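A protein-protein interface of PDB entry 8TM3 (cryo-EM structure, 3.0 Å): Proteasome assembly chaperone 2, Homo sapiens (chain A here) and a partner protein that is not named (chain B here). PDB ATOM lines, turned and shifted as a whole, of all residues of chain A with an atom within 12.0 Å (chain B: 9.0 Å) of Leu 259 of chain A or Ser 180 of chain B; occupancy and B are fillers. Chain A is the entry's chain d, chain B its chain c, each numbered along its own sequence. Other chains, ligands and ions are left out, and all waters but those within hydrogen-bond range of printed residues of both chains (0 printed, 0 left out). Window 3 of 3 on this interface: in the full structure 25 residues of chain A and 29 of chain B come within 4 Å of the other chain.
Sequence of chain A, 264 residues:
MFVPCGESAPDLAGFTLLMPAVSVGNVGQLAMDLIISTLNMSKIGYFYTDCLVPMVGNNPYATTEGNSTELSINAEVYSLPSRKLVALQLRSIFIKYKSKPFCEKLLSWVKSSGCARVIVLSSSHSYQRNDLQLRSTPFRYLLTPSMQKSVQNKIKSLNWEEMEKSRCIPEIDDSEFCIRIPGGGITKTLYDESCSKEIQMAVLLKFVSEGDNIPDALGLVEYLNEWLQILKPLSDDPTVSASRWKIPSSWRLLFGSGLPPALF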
ATOM      1  N   ARG A 252      22.415   8.178 -26.817  1.00  0.00           N
ATOM      2  CA  ARG A 252      21.233   7.834 -26.044  1.00  0.00           C
ATOM      3  C   ARG A 252      20.247   7.125 -26.961  1.00  0.00           C
ATOM      4  O   ARG A 252      20.090   7.506 -28.123  1.00  0.00           O
ATOM      5  CB  ARG A 252      20.596   9.083 -25.427  1.00  0.00           C
ATOM      6  CG  ARG A 252      19.527   8.796 -24.390  1.00  0.00           C
ATOM      7  CD  ARG A 252      18.909  10.082 -23.867  1.00  0.00           C
ATOM      8  NE  ARG A 252      18.140  10.779 -24.893  1.00  0.00           N
ATOM      9  CZ  ARG A 252      16.836  10.635 -25.093  1.00  0.00           C
ATOM     10  NH1 ARG A 252      16.109   9.806 -24.362  1.00  0.00           N
ATOM     11  NH2 ARG A 252      16.247  11.340 -26.055  1.00  0.00           N
ATOM     12  N   LEU A 253      19.588   6.096 -26.431  1.00  0.00           N
ATOM     13  CA  LEU A 253      18.631   5.303 -27.204  1.00  0.00           C
ATOM     14  C   LEU A 253      19.268   4.777 -28.486  1.00  0.00           C
ATOM     15  O   LEU A 253      18.648   4.766 -29.552  1.00  0.00           O
ATOM     16  CB  LEU A 253      17.376   6.117 -27.525  1.00  0.00           C
ATOM     17  CG  LEU A 253      16.608   6.690 -26.333  1.00  0.00           C
ATOM     18  CD1 LEU A 253      15.455   7.554 -26.819  1.00  0.00           C
ATOM     19  CD2 LEU A 253      16.106   5.586 -25.419  1.00  0.00           C
ATOM     20  N   LEU A 254      20.516   4.334 -28.384  1.00  0.00           N
ATOM     21  CA  LEU A 254      21.273   3.880 -29.544  1.00  0.00           C
ATOM     22  C   LEU A 254      21.146   2.383 -29.790  1.00  0.00           C
ATOM     23  O   LEU A 254      21.780   1.869 -30.717  1.00  0.00           O
ATOM     24  CB  LEU A 254      22.755   4.248 -29.389  1.00  0.00           C
ATOM     25  CG  LEU A 254      23.611   3.474 -28.380  1.00  0.00           C
ATOM     26  CD1 LEU A 254      25.066   3.886 -28.525  1.00  0.00           C
ATOM     27  CD2 LEU A 254      23.146   3.687 -26.949  1.00  0.00           C
ATOM     28  N   PHE A 255      20.352   1.672 -28.989  1.00  0.00           N
ATOM     29  CA  PHE A 255      20.203   0.232 -29.143  1.00  0.00           C
ATOM     30  C   PHE A 255      18.770  -0.266 -29.038  1.00  0.00           C
ATOM     31  O   PHE A 255      18.542  -1.461 -29.251  1.00  0.00           O
ATOM     32  CB  PHE A 255      21.052  -0.505 -28.095  1.00  0.00           C
ATOM     33  N   GLY A 256      17.806   0.590 -28.725  1.00  0.00           N
ATOM     34  CA  GLY A 256      16.438   0.134 -28.568  1.00  0.00           C
ATOM     35  C   GLY A 256      15.496   1.309 -28.450  1.00  0.00           C
ATOM     36  O   GLY A 256      15.909   2.473 -28.450  1.00  0.00           O
ATOM     37  N   SER A 257      14.208   0.984 -28.353  1.00  0.00           N
ATOM     38  CA  SER A 257      13.143   1.977 -28.280  1.00  0.00           C
ATOM     39  C   SER A 257      12.138   1.612 -27.197  1.00  0.00           C
ATOM     40  O   SER A 257      10.929   1.802 -27.356  1.00  0.00           O
ATOM     41  CB  SER A 257      12.442   2.124 -29.627  1.00  0.00           C
ATOM     42  OG  SER A 257      11.816   3.390 -29.739  1.00  0.00           O
ATOM     43  N   GLY A 258      12.619   1.084 -26.084  1.00  0.00           N
ATOM     44  CA  GLY A 258      11.754   0.790 -24.960  1.00  0.00           C
ATOM     45  C   GLY A 258      11.306  -0.659 -24.932  1.00  0.00           C
ATOM     46  O   GLY A 258      11.304  -1.363 -25.949  1.00  0.00           O
ATOM     47  N   LEU A 259      10.917  -1.114 -23.747  1.00  0.00           N
ATOM     48  CA  LEU A 259      10.468  -2.488 -23.559  1.00  0.00           C
ATOM     49  C   LEU A 259       8.960  -2.576 -23.760  1.00  0.00           C
ATOM     50  O   LEU A 259       8.211  -1.969 -22.986  1.00  0.00           O
ATOM     51  CB  LEU A 259      10.833  -2.968 -22.158  1.00  0.00           C
ATOM     52  CG  LEU A 259      10.847  -4.469 -21.841  1.00  0.00           C
ATOM     53  CD1 LEU A 259      11.315  -5.305 -23.015  1.00  0.00           C
ATOM     54  CD2 LEU A 259      11.717  -4.733 -20.622  1.00  0.00           C
ATOM     55  N   PRO A 260       8.471  -3.305 -24.760  1.00  0.00           N
ATOM     56  CA  PRO A 260       7.022  -3.498 -24.888  1.00  0.00           C
ATOM     57  C   PRO A 260       6.469  -4.239 -23.686  1.00  0.00           C
ATOM     58  O   PRO A 260       6.954  -5.328 -23.344  1.00  0.00           O
ATOM     59  CB  PRO A 260       6.882  -4.328 -26.175  1.00  0.00           C
ATOM     60  CG  PRO A 260       8.149  -4.103 -26.917  1.00  0.00           C
ATOM     61  CD  PRO A 260       9.203  -3.927 -25.876  1.00  0.00           C
ATOM     62  N   PRO A 261       5.456  -3.687 -23.012  1.00  0.00           N
ATOM     63  CA  PRO A 261       4.988  -4.317 -21.765  1.00  0.00           C
ATOM     64  C   PRO A 261       4.470  -5.733 -21.944  1.00  0.00           C
ATOM     65  O   PRO A 261       4.658  -6.566 -21.049  1.00  0.00           O
ATOM     66  CB  PRO A 261       3.879  -3.367 -21.291  1.00  0.00           C
ATOM     67  CG  PRO A 261       3.420  -2.669 -22.520  1.00  0.00           C
ATOM     68  CD  PRO A 261       4.631  -2.525 -23.387  1.00  0.00           C
ATOM     69  N   ALA A 262       3.823  -6.037 -23.071  1.00  0.00           N
ATOM     70  CA  ALA A 262       3.213  -7.351 -23.239  1.00  0.00           C
ATOM     71  C   ALA A 262       4.244  -8.457 -23.413  1.00  0.00           C
ATOM     72  O   ALA A 262       3.935  -9.621 -23.138  1.00  0.00           O
ATOM     73  CB  ALA A 262       2.262  -7.341 -24.436  1.00  0.00           C
ATOM     74  N   LEU A 263       5.457  -8.127 -23.861  1.00  0.00           N
ATOM     75  CA  LEU A 263       6.471  -9.157 -24.065  1.00  0.00           C
ATOM     76  C   LEU A 263       6.797  -9.870 -22.760  1.00  0.00           C
ATOM     77  O   LEU A 263       6.924 -11.100 -22.725  1.00  0.00           O
ATOM     78  CB  LEU A 263       7.735  -8.538 -24.665  1.00  0.00           C
ATOM     79  CG  LEU A 263       7.919  -8.674 -26.177  1.00  0.00           C
ATOM     80  CD1 LEU A 263       9.123  -7.866 -26.630  1.00  0.00           C
ATOM     81  CD2 LEU A 263       8.076 -10.130 -26.579  1.00  0.00           C
ATOM     82  N   PHE A 264       6.936  -9.115 -21.676  1.00  0.00           N
ATOM     83  CA  PHE A 264       7.280  -9.692 -20.383  1.00  0.00           C
ATOM     84  C   PHE A 264       6.136  -9.527 -19.388  1.00  0.00           C
ATOM     85  O   PHE A 264       5.142 -10.252 -19.443  1.00  0.00           O
ATOM     86  CB  PHE A 264       8.554  -9.051 -19.833  1.00  0.00           C
ATOM     87  CG  PHE A 264       9.792  -9.409 -20.602  1.00  0.00           C
ATOM     88  CD1 PHE A 264      10.127  -8.726 -21.759  1.00  0.00           C
ATOM     89  CD2 PHE A 264      10.620 -10.431 -20.173  1.00  0.00           C
ATOM     90  CE1 PHE A 264      11.263  -9.053 -22.470  1.00  0.00           C
ATOM     91  CE2 PHE A 264      11.757 -10.763 -20.880  1.00  0.00           C
ATOM     92  CZ  PHE A 264      12.079 -10.074 -22.030  1.00  0.00           C
ATOM     93  N   VAL B 172       5.530   5.896 -36.490  1.00  0.00           N
ATOM     94  CA  VAL B 172       5.818   5.995 -35.063  1.00  0.00           C
ATOM     95  C   VAL B 172       7.079   5.219 -34.715  1.00  0.00           C
ATOM     96  O   VAL B 172       7.864   5.646 -33.860  1.00  0.00           O
ATOM     97  CB  VAL B 172       4.610   5.503 -34.241  1.00  0.00           C
ATOM     98  CG1 VAL B 172       4.919   5.566 -32.754  1.00  0.00           C
ATOM     99  CG2 VAL B 172       3.374   6.327 -34.567  1.00  0.00           C
ATOM    100  N   THR B 173       7.297   4.071 -35.361  1.00  0.00           N
ATOM    101  CA  THR B 173       8.478   3.268 -35.061  1.00  0.00           C
ATOM    102  C   THR B 173       9.763   4.048 -35.299  1.00  0.00           C
ATOM    103  O   THR B 173      10.753   3.842 -34.588  1.00  0.00           O
ATOM    104  CB  THR B 173       8.475   1.994 -35.905  1.00  0.00           C
ATOM    105  OG1 THR B 173       8.473   2.339 -37.295  1.00  0.00           O
ATOM    106  CG2 THR B 173       7.251   1.148 -35.590  1.00  0.00           C
ATOM    107  N   TYR B 175      10.267   7.091 -34.617  1.00  0.00           N
ATOM    108  CA  TYR B 175      10.463   7.974 -33.476  1.00  0.00           C
ATOM    109  C   TYR B 175      11.261   7.270 -32.387  1.00  0.00           C
ATOM    110  O   TYR B 175      10.775   6.313 -31.776  1.00  0.00           O
ATOM    111  CB  TYR B 175       9.111   8.433 -32.927  1.00  0.00           C
ATOM    112  CG  TYR B 175       9.198   9.443 -31.806  1.00  0.00           C
ATOM    113  CD1 TYR B 175       9.788  10.682 -32.004  1.00  0.00           C
ATOM    114  CD2 TYR B 175       8.689   9.155 -30.549  1.00  0.00           C
ATOM    115  CE1 TYR B 175       9.863  11.608 -30.982  1.00  0.00           C
ATOM    116  CE2 TYR B 175       8.762  10.072 -29.521  1.00  0.00           C
ATOM    117  CZ  TYR B 175       9.352  11.296 -29.742  1.00  0.00           C
ATOM    118  OH  TYR B 175       9.427  12.213 -28.719  1.00  0.00           O
ATOM    119  N   LYS B 176      12.483   7.731 -32.136  1.00  0.00           N
ATOM    120  CA  LYS B 176      13.311   7.161 -31.082  1.00  0.00           C
ATOM    121  C   LYS B 176      12.855   7.720 -29.740  1.00  0.00           C
ATOM    122  O   LYS B 176      12.986   8.922 -29.485  1.00  0.00           O
ATOM    123  CB  LYS B 176      14.783   7.480 -31.332  1.00  0.00           C
ATOM    124  CG  LYS B 176      15.422   6.710 -32.487  1.00  0.00           C
ATOM    125  CD  LYS B 176      15.251   5.199 -32.387  1.00  0.00           C
ATOM    126  CE  LYS B 176      15.566   4.662 -30.998  1.00  0.00           C
ATOM    127  NZ  LYS B 176      15.275   3.210 -30.901  1.00  0.00           N
ATOM    128  N   THR B 177      12.322   6.851 -28.883  1.00  0.00           N
ATOM    129  CA  THR B 177      11.708   7.262 -27.630  1.00  0.00           C
ATOM    130  C   THR B 177      12.232   6.411 -26.484  1.00  0.00           C
ATOM    131  O   THR B 177      12.588   5.244 -26.667  1.00  0.00           O
ATOM    132  CB  THR B 177      10.181   7.139 -27.684  1.00  0.00           C
ATOM    133  OG1 THR B 177       9.642   7.237 -26.361  1.00  0.00           O
ATOM    134  CG2 THR B 177       9.774   5.806 -28.298  1.00  0.00           C
ATOM    135  N   SER B 178      12.271   7.013 -25.294  1.00  0.00           N
ATOM    136  CA  SER B 178      12.711   6.279 -24.112  1.00  0.00           C
ATOM    137  C   SER B 178      11.749   5.148 -23.775  1.00  0.00           C
ATOM    138  O   SER B 178      12.179   4.037 -23.439  1.00  0.00           O
ATOM    139  CB  SER B 178      12.851   7.232 -22.926  1.00  0.00           C
ATOM    140  OG  SER B 178      12.942   6.515 -21.708  1.00  0.00           O
ATOM    141  N   GLU B 179      10.448   5.407 -23.856  1.00  0.00           N
ATOM    142  CA  GLU B 179       9.442   4.408 -23.538  1.00  0.00           C
ATOM    143  C   GLU B 179       9.104   3.605 -24.794  1.00  0.00           C
ATOM    144  O   GLU B 179       9.673   3.817 -25.867  1.00  0.00           O
ATOM    145  CB  GLU B 179       8.205   5.080 -22.944  1.00  0.00           C
ATOM    146  N   SER B 180       8.164   2.673 -24.669  1.00  0.00           N
ATOM    147  CA  SER B 180       7.760   1.856 -25.800  1.00  0.00           C
ATOM    148  C   SER B 180       6.995   2.696 -26.819  1.00  0.00           C
ATOM    149  O   SER B 180       6.295   3.654 -26.477  1.00  0.00           O
ATOM    150  CB  SER B 180       6.894   0.684 -25.336  1.00  0.00           C
ATOM    151  OG  SER B 180       5.672   1.141 -24.785  1.00  0.00           O
ATOM    152  N   THR B 181       7.138   2.321 -28.091  1.00  0.00           N
ATOM    153  CA  THR B 181       6.478   3.056 -29.161  1.00  0.00           C
ATOM    154  C   THR B 181       4.961   3.021 -29.039  1.00  0.00           C
ATOM    155  O   THR B 181       4.290   3.923 -29.550  1.00  0.00           O
ATOM    156  CB  THR B 181       6.892   2.495 -30.522  1.00  0.00           C
ATOM    157  OG1 THR B 181       6.535   1.109 -30.599  1.00  0.00           O
ATOM    158  CG2 THR B 181       8.392   2.643 -30.732  1.00  0.00           C
ATOM    159  N   GLY B 182       4.404   2.004 -28.378  1.00  0.00           N
ATOM    160  CA  GLY B 182       2.961   1.909 -28.263  1.00  0.00           C
ATOM    161  C   GLY B 182       2.359   2.964 -27.357  1.00  0.00           C
ATOM    162  O   GLY B 182       1.176   3.293 -27.486  1.00  0.00           O
ATOM    163  N   SER B 183       3.151   3.506 -26.431  1.00  0.00           N
ATOM    164  CA  SER B 183       2.653   4.525 -25.517  1.00  0.00           C
ATOM    165  C   SER B 183       2.517   5.891 -26.173  1.00  0.00           C
ATOM    166  O   SER B 183       1.795   6.746 -25.650  1.00  0.00           O
ATOM    167  CB  SER B 183       3.577   4.635 -24.303  1.00  0.00           C
ATOM    168  OG  SER B 183       2.862   5.061 -23.155  1.00  0.00           O
ATOM    169  N   LEU B 184       3.188   6.117 -27.299  1.00  0.00           N
ATOM    170  CA  LEU B 184       3.158   7.422 -27.932  1.00  0.00           C
ATOM    171  C   LEU B 184       1.770   7.708 -28.505  1.00  0.00           C
ATOM    172  O   LEU B 184       1.048   6.785 -28.891  1.00  0.00           O
ATOM    173  CB  LEU B 184       4.195   7.496 -29.048  1.00  0.00           C
ATOM    174  CG  LEU B 184       5.639   7.198 -28.643  1.00  0.00           C
ATOM    175  CD1 LEU B 184       6.430   6.701 -29.843  1.00  0.00           C
ATOM    176  CD2 LEU B 184       6.291   8.427 -28.038  1.00  0.00           C
ATOM    177  N   PRO B 185       1.368   8.979 -28.570  1.00  0.00           N
ATOM    178  CA  PRO B 185       0.127   9.309 -29.279  1.00  0.00           C
ATOM    179  C   PRO B 185       0.243   8.947 -30.750  1.00  0.00           C
ATOM    180  O   PRO B 185       1.303   9.079 -31.365  1.00  0.00           O
ATOM    181  CB  PRO B 185      -0.014  10.824 -29.078  1.00  0.00           C
ATOM    182  CG  PRO B 185       0.928  11.172 -27.972  1.00  0.00           C
ATOM    183  CD  PRO B 185       2.039  10.182 -28.054  1.00  0.00           C
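OG1 of Thr 177 of chain B lies within hydrogen-bond range of N of Glu 179 of chain B (3.2 Å).
Phe 255 of chain A touches none of the printed residues of chain B. Of the printed residues of chain B, Gly 256 of chain A touches Lys 176 (2.6 Å). Gly 258 of chain A touches just these residues of chain B: Ser 178 and Glu 179. Of the printed residues of chain B, Leu 259 of chain A touches Ser 180. Phe 264 of chain A touches none of the printed residues of chain B. Of the printed residues of chain A, Tyr 175 of chain B touches Ser 257 (3.7 Å). Of the printed residues of chain A, Lys 176 of chain B touches Leu 253, Gly 256 and Ser 257. Ser 178 of chain B touches just these residues of chain A: Leu 253 (3.6 Å) and Gly 258 (3.6 Å). Glu 179 of chain B touches two residues of chain A. Of the printed residues of chain A, Ser 180 of chain B touches Ser 257 (3.5 Å) and Leu 259 (3.8 Å). Printed residues of chain A within 4 Å of Thr 181 of chain B: Ser 257. No residue of chain A comes within 4 Å of Gly 182 of chain B. No residue of chain A comes within 4 Å of Ser 183 of chain B. No residue of chain A comes within 4 Å of Leu 184 of chain B.
Among the printed residues, pairs that only touch across the chains: Leu 253 of chain A with Lys 176 of chain B (3.4 Å), Leu 253 of chain A with Thr 177 of chain B (3.4 Å), Leu 253 of chain A with Ser 178 of chain B (3.6 Å), Ser 257 of chain A with Tyr 175 of chain B (3.7 Å), Ser 257 of chain A with Lys 176 of chain B (3.3 Å), Ser 257 of chain A with Thr 177 of chain B (3.5 Å), Ser 257 of chain A with Ser 180 of chain B (3.5 Å), Ser 257 of chain A with Thr 181 of chain B (3.6 Å), Gly 258 of chain A with Ser 178 of chain B (3.6 Å), Gly 258 of chain A with Glu 179 of chain B (3.8 Å) and Leu 259 of chain A with Ser 180 of chain B (3.8 Å).
The backbone carbonyl oxygen (O) of Gly 256 of chain A is in hydrogen-bond range of the side-chain amino group (NZ) of Lys 176 of chain B (2.6 Å). O of Ser 257 of chain A lies close to O of Glu 179 of chain B (2.8 Å).
Printed residues of chain B that touch a printed residue of chain A: Tyr 175, Lys 176, Thr 177, Ser 178, Glu 179, Ser 180 and Thr 181. Of the 13 printed residues of chain A, 5 touch a printed residue of chain B. Hydrophobic or aromatic side chains of chain A within 4 Å of the printed part of chain B: Leu 253.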
